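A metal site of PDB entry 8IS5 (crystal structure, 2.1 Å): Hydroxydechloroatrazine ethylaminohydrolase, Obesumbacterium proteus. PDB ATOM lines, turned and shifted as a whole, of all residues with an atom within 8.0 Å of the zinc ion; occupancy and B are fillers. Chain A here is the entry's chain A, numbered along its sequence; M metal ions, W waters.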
ATOM      1  N   HIS A  68     -15.384  -0.174 -22.039  1.00  0.00           N
ATOM      2  CA  HIS A  68     -14.354  -1.187 -21.792  1.00  0.00           C
ATOM      3  C   HIS A  68     -13.047  -0.744 -22.439  1.00  0.00           C
ATOM      4  O   HIS A  68     -13.038  -0.317 -23.595  1.00  0.00           O
ATOM      5  CB  HIS A  68     -14.803  -2.557 -22.327  1.00  0.00           C
ATOM      6  CG  HIS A  68     -13.885  -3.667 -21.932  1.00  0.00           C
ATOM      7  ND1 HIS A  68     -13.676  -4.022 -20.623  1.00  0.00           N
ATOM      8  CD2 HIS A  68     -13.093  -4.473 -22.672  1.00  0.00           C
ATOM      9  CE1 HIS A  68     -12.806  -5.011 -20.565  1.00  0.00           C
ATOM     10  NE2 HIS A  68     -12.434  -5.311 -21.800  1.00  0.00           N
ATOM     11  N   HIS A  69     -11.941  -0.913 -21.710  1.00  0.00           N
ATOM     12  CA  HIS A  69     -10.635  -0.468 -22.191  1.00  0.00           C
ATOM     13  C   HIS A  69      -9.555  -1.145 -21.364  1.00  0.00           C
ATOM     14  O   HIS A  69      -9.827  -1.781 -20.335  1.00  0.00           O
ATOM     15  CB  HIS A  69     -10.489   1.054 -22.081  1.00  0.00           C
ATOM     16  CG  HIS A  69      -9.640   1.661 -23.160  1.00  0.00           C
ATOM     17  ND1 HIS A  69      -8.450   1.119 -23.580  1.00  0.00           N
ATOM     18  CD2 HIS A  69      -9.819   2.787 -23.891  1.00  0.00           C
ATOM     19  CE1 HIS A  69      -7.934   1.874 -24.525  1.00  0.00           C
ATOM     20  NE2 HIS A  69      -8.752   2.901 -24.740  1.00  0.00           N
ATOM     21  N   HIS A  70      -8.307  -1.040 -21.853  1.00  0.00           N
ATOM     22  CA  HIS A  70      -7.100  -1.319 -21.072  1.00  0.00           C
ATOM     23  C   HIS A  70      -6.111  -0.257 -21.523  1.00  0.00           C
ATOM     24  O   HIS A  70      -5.269  -0.510 -22.394  1.00  0.00           O
ATOM     25  CB  HIS A  70      -6.548  -2.727 -21.287  1.00  0.00           C
ATOM     26  CG  HIS A  70      -7.558  -3.800 -21.065  1.00  0.00           C
ATOM     27  ND1 HIS A  70      -8.155  -4.003 -19.837  1.00  0.00           N
ATOM     28  CD2 HIS A  70      -8.104  -4.691 -21.911  1.00  0.00           C
ATOM     29  CE1 HIS A  70      -9.005  -5.005 -19.939  1.00  0.00           C
ATOM     30  NE2 HIS A  70      -8.987  -5.452 -21.172  1.00  0.00           N
ATOM     31  N   GLN A  73      -2.381  -0.562 -22.368  1.00  0.00           N
ATOM     32  CA  GLN A  73      -1.933  -1.191 -23.609  1.00  0.00           C
ATOM     33  C   GLN A  73      -1.683  -0.203 -24.736  1.00  0.00           C
ATOM     34  O   GLN A  73      -1.085  -0.584 -25.741  1.00  0.00           O
ATOM     35  CB  GLN A  73      -2.949  -2.258 -24.057  1.00  0.00           C
ATOM     36  CG  GLN A  73      -3.219  -3.324 -22.980  1.00  0.00           C
ATOM     37  CD  GLN A  73      -4.235  -4.359 -23.394  1.00  0.00           C
ATOM     38  OE1 GLN A  73      -4.829  -4.272 -24.475  1.00  0.00           O
ATOM     39  NE2 GLN A  73      -4.445  -5.363 -22.554  1.00  0.00           N
ATOM     40  N   TRP A  90      -0.593 -14.225 -27.962  1.00  0.00           N
ATOM     41  CA  TRP A  90      -0.829 -12.810 -27.692  1.00  0.00           C
ATOM     42  C   TRP A  90      -0.537 -12.474 -26.238  1.00  0.00           C
ATOM     43  O   TRP A  90       0.325 -11.635 -25.934  1.00  0.00           O
ATOM     44  CB  TRP A  90      -2.279 -12.465 -28.059  1.00  0.00           C
ATOM     45  CG  TRP A  90      -2.686 -11.010 -27.967  1.00  0.00           C
ATOM     46  CD1 TRP A  90      -2.595 -10.073 -28.953  1.00  0.00           C
ATOM     47  CD2 TRP A  90      -3.284 -10.345 -26.834  1.00  0.00           C
ATOM     48  NE1 TRP A  90      -3.068  -8.852 -28.499  1.00  0.00           N
ATOM     49  CE2 TRP A  90      -3.502  -8.994 -27.209  1.00  0.00           C
ATOM     50  CE3 TRP A  90      -3.638 -10.741 -25.540  1.00  0.00           C
ATOM     51  CZ2 TRP A  90      -4.070  -8.049 -26.333  1.00  0.00           C
ATOM     52  CZ3 TRP A  90      -4.199  -9.810 -24.683  1.00  0.00           C
ATOM     53  CH2 TRP A  90      -4.412  -8.472 -25.078  1.00  0.00           C
ATOM     54  N   HIS A 128     -10.045  -0.715 -17.478  1.00  0.00           N
ATOM     55  CA  HIS A 128      -9.933  -1.996 -16.797  1.00  0.00           C
ATOM     56  C   HIS A 128      -8.439  -2.287 -16.590  1.00  0.00           C
ATOM     57  O   HIS A 128      -7.846  -3.168 -17.211  1.00  0.00           O
ATOM     58  CB  HIS A 128     -10.651  -3.094 -17.582  1.00  0.00           C
ATOM     59  CG  HIS A 128     -10.805  -4.389 -16.844  1.00  0.00           C
ATOM     60  ND1 HIS A 128     -11.307  -5.528 -17.441  1.00  0.00           N
ATOM     61  CD2 HIS A 128     -10.520  -4.724 -15.570  1.00  0.00           C
ATOM     62  CE1 HIS A 128     -11.336  -6.503 -16.548  1.00  0.00           C
ATOM     63  NE2 HIS A 128     -10.864  -6.039 -15.410  1.00  0.00           N
ATOM     64  N   TYR A 130      -5.699  -4.079 -14.897  1.00  0.00           N
ATOM     65  CA  TYR A 130      -5.663  -5.306 -14.098  1.00  0.00           C
ATOM     66  C   TYR A 130      -4.248  -5.786 -13.804  1.00  0.00           C
ATOM     67  O   TYR A 130      -4.096  -6.878 -13.248  1.00  0.00           O
ATOM     68  CB  TYR A 130      -6.472  -6.420 -14.780  1.00  0.00           C
ATOM     69  CG  TYR A 130      -5.984  -6.860 -16.147  1.00  0.00           C
ATOM     70  CD1 TYR A 130      -5.015  -7.855 -16.300  1.00  0.00           C
ATOM     71  CD2 TYR A 130      -6.502  -6.281 -17.299  1.00  0.00           C
ATOM     72  CE1 TYR A 130      -4.592  -8.258 -17.560  1.00  0.00           C
ATOM     73  CE2 TYR A 130      -6.088  -6.658 -18.534  1.00  0.00           C
ATOM     74  CZ  TYR A 130      -5.134  -7.645 -18.676  1.00  0.00           C
ATOM     75  OH  TYR A 130      -4.739  -8.011 -19.945  1.00  0.00           O
ATOM     76  N   CYS A 207     -10.197  -9.907 -13.660  1.00  0.00           N
ATOM     77  CA  CYS A 207     -10.004  -9.882 -15.106  1.00  0.00           C
ATOM     78  C   CYS A 207     -11.020 -10.791 -15.810  1.00  0.00           C
ATOM     79  O   CYS A 207     -11.552 -10.445 -16.864  1.00  0.00           O
ATOM     80  CB  CYS A 207      -8.567 -10.282 -15.472  1.00  0.00           C
ATOM     81  SG  CYS A 207      -8.208 -10.009 -17.258  1.00  0.00           S
ATOM     82  N   HIS A 232     -17.402  -5.628 -12.994  1.00  0.00           N
ATOM     83  CA  HIS A 232     -17.059  -5.713 -14.415  1.00  0.00           C
ATOM     84  C   HIS A 232     -16.076  -6.856 -14.635  1.00  0.00           C
ATOM     85  O   HIS A 232     -15.194  -7.075 -13.800  1.00  0.00           O
ATOM     86  CB  HIS A 232     -16.457  -4.366 -14.882  1.00  0.00           C
ATOM     87  CG  HIS A 232     -16.087  -4.317 -16.334  1.00  0.00           C
ATOM     88  ND1 HIS A 232     -16.966  -4.639 -17.346  1.00  0.00           N
ATOM     89  CD2 HIS A 232     -14.940  -3.942 -16.940  1.00  0.00           C
ATOM     90  CE1 HIS A 232     -16.375  -4.481 -18.515  1.00  0.00           C
ATOM     91  NE2 HIS A 232     -15.146  -4.046 -18.294  1.00  0.00           N
ATOM     92  N   THR A 233     -16.216  -7.578 -15.742  1.00  0.00           N
ATOM     93  CA  THR A 233     -15.261  -8.647 -16.052  1.00  0.00           C
ATOM     94  C   THR A 233     -15.429  -9.044 -17.511  1.00  0.00           C
ATOM     95  O   THR A 233     -16.398  -8.656 -18.172  1.00  0.00           O
ATOM     96  CB  THR A 233     -15.443  -9.849 -15.115  1.00  0.00           C
ATOM     97  OG1 THR A 233     -14.289 -10.683 -15.185  1.00  0.00           O
ATOM     98  CG2 THR A 233     -16.681 -10.663 -15.490  1.00  0.00           C
ATOM     99  N   HIS A 234     -14.471  -9.847 -17.997  1.00  0.00           N
ATOM    100  CA  HIS A 234     -14.569 -10.466 -19.318  1.00  0.00           C
ATOM    101  C   HIS A 234     -15.415 -11.727 -19.222  1.00  0.00           C
ATOM    102  O   HIS A 234     -15.160 -12.596 -18.366  1.00  0.00           O
ATOM    103  CB  HIS A 234     -13.188 -10.840 -19.857  1.00  0.00           C
ATOM    104  CG  HIS A 234     -12.257  -9.682 -20.080  1.00  0.00           C
ATOM    105  ND1 HIS A 234     -11.155  -9.449 -19.288  1.00  0.00           N
ATOM    106  CD2 HIS A 234     -12.223  -8.740 -21.057  1.00  0.00           C
ATOM    107  CE1 HIS A 234     -10.506  -8.396 -19.734  1.00  0.00           C
ATOM    108  NE2 HIS A 234     -11.126  -7.948 -20.814  1.00  0.00           N
ATOM    109  N   GLU A 237     -15.871 -14.640 -24.139  1.00  0.00           N
ATOM    110  CA  GLU A 237     -15.243 -13.900 -25.233  1.00  0.00           C
ATOM    111  C   GLU A 237     -15.000 -14.786 -26.447  1.00  0.00           C
ATOM    112  O   GLU A 237     -15.056 -14.283 -27.578  1.00  0.00           O
ATOM    113  CB  GLU A 237     -13.931 -13.274 -24.758  1.00  0.00           C
ATOM    114  CG  GLU A 237     -13.223 -12.461 -25.859  1.00  0.00           C
ATOM    115  CD  GLU A 237     -11.969 -11.762 -25.365  1.00  0.00           C
ATOM    116  OE1 GLU A 237     -11.666 -11.890 -24.150  1.00  0.00           O
ATOM    117  OE2 GLU A 237     -11.312 -11.085 -26.187  1.00  0.00           O
ATOM    118  N   ALA A 270     -17.835  -7.707 -20.314  1.00  0.00           N
ATOM    119  CA  ALA A 270     -17.209  -7.393 -21.593  1.00  0.00           C
ATOM    120  C   ALA A 270     -17.300  -8.561 -22.576  1.00  0.00           C
ATOM    121  O   ALA A 270     -17.155  -9.730 -22.184  1.00  0.00           O
ATOM    122  CB  ALA A 270     -15.734  -7.013 -21.394  1.00  0.00           C
ATOM    123  N   HIS A 271     -17.569  -8.234 -23.838  1.00  0.00           N
ATOM    124  CA  HIS A 271     -17.544  -9.137 -24.999  1.00  0.00           C
ATOM    125  C   HIS A 271     -18.818  -9.947 -25.128  1.00  0.00           C
ATOM    126  O   HIS A 271     -19.678  -9.604 -25.958  1.00  0.00           O
ATOM    127  CB  HIS A 271     -16.317 -10.069 -24.974  1.00  0.00           C
ATOM    128  CG  HIS A 271     -15.018  -9.333 -24.965  1.00  0.00           C
ATOM    129  ND1 HIS A 271     -14.665  -8.416 -25.935  1.00  0.00           N
ATOM    130  CD2 HIS A 271     -13.972  -9.378 -24.104  1.00  0.00           C
ATOM    131  CE1 HIS A 271     -13.467  -7.923 -25.666  1.00  0.00           C
ATOM    132  NE2 HIS A 271     -13.026  -8.496 -24.554  1.00  0.00           N
ATOM    133  N   CYS A 293     -17.583  -5.045 -28.022  1.00  0.00           N
ATOM    134  CA  CYS A 293     -16.275  -4.579 -28.496  1.00  0.00           C
ATOM    135  C   CYS A 293     -15.995  -5.138 -29.896  1.00  0.00           C
ATOM    136  O   CYS A 293     -15.198  -6.068 -30.040  1.00  0.00           O
ATOM    137  CB  CYS A 293     -15.170  -4.996 -27.527  1.00  0.00           C
ATOM    138  SG  CYS A 293     -15.350  -4.310 -25.881  1.00  0.00           S
ATOM    139  N   SER A 296     -12.087  -5.282 -31.436  1.00  0.00           N
ATOM    140  CA  SER A 296     -11.325  -6.307 -30.740  1.00  0.00           C
ATOM    141  C   SER A 296     -11.804  -7.705 -31.113  1.00  0.00           C
ATOM    142  O   SER A 296     -10.987  -8.621 -31.312  1.00  0.00           O
ATOM    143  CB  SER A 296     -11.436  -6.120 -29.222  1.00  0.00           C
ATOM    144  OG  SER A 296     -10.868  -7.217 -28.515  1.00  0.00           O
ATOM    145  N   LEU A 300      -8.957 -10.059 -32.906  1.00  0.00           N
ATOM    146  CA  LEU A 300      -8.539 -11.281 -32.217  1.00  0.00           C
ATOM    147  C   LEU A 300      -9.287 -12.503 -32.719  1.00  0.00           C
ATOM    148  O   LEU A 300      -9.148 -13.580 -32.117  1.00  0.00           O
ATOM    149  CB  LEU A 300      -8.738 -11.139 -30.702  1.00  0.00           C
ATOM    150  CG  LEU A 300      -7.672 -10.338 -29.930  1.00  0.00           C
ATOM    151  CD1 LEU A 300      -8.058 -10.200 -28.457  1.00  0.00           C
ATOM    152  CD2 LEU A 300      -6.326 -11.020 -30.031  1.00  0.00           C
ATOM    153  N   VAL A 321     -14.027   0.140 -26.827  1.00  0.00           N
ATOM    154  CA  VAL A 321     -12.958  -0.087 -27.800  1.00  0.00           C
ATOM    155  C   VAL A 321     -12.051  -1.227 -27.363  1.00  0.00           C
ATOM    156  O   VAL A 321     -11.351  -1.791 -28.211  1.00  0.00           O
ATOM    157  CB  VAL A 321     -12.144   1.187 -28.063  1.00  0.00           C
ATOM    158  CG1 VAL A 321     -13.022   2.225 -28.728  1.00  0.00           C
ATOM    159  CG2 VAL A 321     -11.556   1.742 -26.781  1.00  0.00           C
ATOM    160  N   ASP A 322     -12.034  -1.552 -26.070  1.00  0.00           N
ATOM    161  CA  ASP A 322     -11.113  -2.560 -25.513  1.00  0.00           C
ATOM    162  C   ASP A 322      -9.683  -2.011 -25.530  1.00  0.00           C
ATOM    163  O   ASP A 322      -9.425  -0.936 -26.065  1.00  0.00           O
ATOM    164  CB  ASP A 322     -11.187  -3.883 -26.272  1.00  0.00           C
ATOM    165  CG  ASP A 322     -10.768  -5.069 -25.419  1.00  0.00           C
ATOM    166  OD1 ASP A 322     -10.399  -4.892 -24.236  1.00  0.00           O
ATOM    167  OD2 ASP A 322     -10.760  -6.187 -25.953  1.00  0.00           O
ATOM    168  N   GLY A 323      -8.750  -2.770 -24.935  1.00  0.00           N
ATOM    169  CA  GLY A 323      -7.387  -2.305 -24.860  1.00  0.00           C
ATOM    170  C   GLY A 323      -6.764  -2.107 -26.235  1.00  0.00           C
ATOM    171  O   GLY A 323      -7.121  -2.772 -27.204  1.00  0.00           O
ATOM    172  N   SER A 326      -5.496  -4.865 -28.473  1.00  0.00           N
ATOM    173  CA  SER A 326      -6.440  -5.719 -29.186  1.00  0.00           C
ATOM    174  C   SER A 326      -7.524  -4.849 -29.829  1.00  0.00           C
ATOM    175  O   SER A 326      -8.705  -4.934 -29.501  1.00  0.00           O
ATOM    176  CB  SER A 326      -7.028  -6.784 -28.268  1.00  0.00           C
ATOM    177  OG  SER A 326      -7.884  -6.215 -27.310  1.00  0.00           O
HETATM  178 ZN    ZN M   1     -10.576  -6.427 -22.356  1.00  0.00          ZN
HETATM  179  O   HOH W   1     -10.450  -7.766 -23.867  1.00  0.00           O
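The side-chain carboxylate (OD2) of Asp 322 sits at hydrogen-bond distance from the side-chain hydroxyl (OG) of Ser 326 (3.2 Å).
OG of Ser 296 sits at hydrogen-bond distance from OD2 of Asp 322 (2.8 Å).
The backbone NH (N) of Val 321 lies within hydrogen-bond range of the backbone carbonyl oxygen (O) of His 68 (3.4 Å).
A ring nitrogen (ND1) of His 70 sits at hydrogen-bond distance from the backbone carbonyl oxygen (O) of His 128, at 2.8 Å.
A ring nitrogen (ND1) of His 68 lies within hydrogen-bond range of a ring nitrogen (NE2) of His 232 (2.8 Å).
A ring nitrogen (ND1) of His 234 lies within hydrogen-bond range of the backbone carbonyl oxygen of Cys 207, 2.7 Å away.
The backbone carbonyl oxygen (O) of Asp 322 lies within hydrogen-bond range of a ring nitrogen (ND1) of His 69.
His 271 touches the zinc ion (NE2 to ZN, 3.9 Å).
Of the 21 residues printed, 5 come within 4 Å of the zinc ion.
The nearest printed residue that does not touch the zinc ion is Gly 323 (4.8 Å).
The zinc ion is bound by water W1 (2.0 Å), NE2 of His 70 (2.2 Å), NE2 of His 234 (2.2 Å), NE2 of His 68 (2.2 Å) and OD1 of Asp 322 (2.4 Å).
Water W1 lies within hydrogen-bond range of the side-chain carboxylate (OD2) of Asp 322 (2.6 Å) and a ring nitrogen (NE2) of His 271 (2.8 Å).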
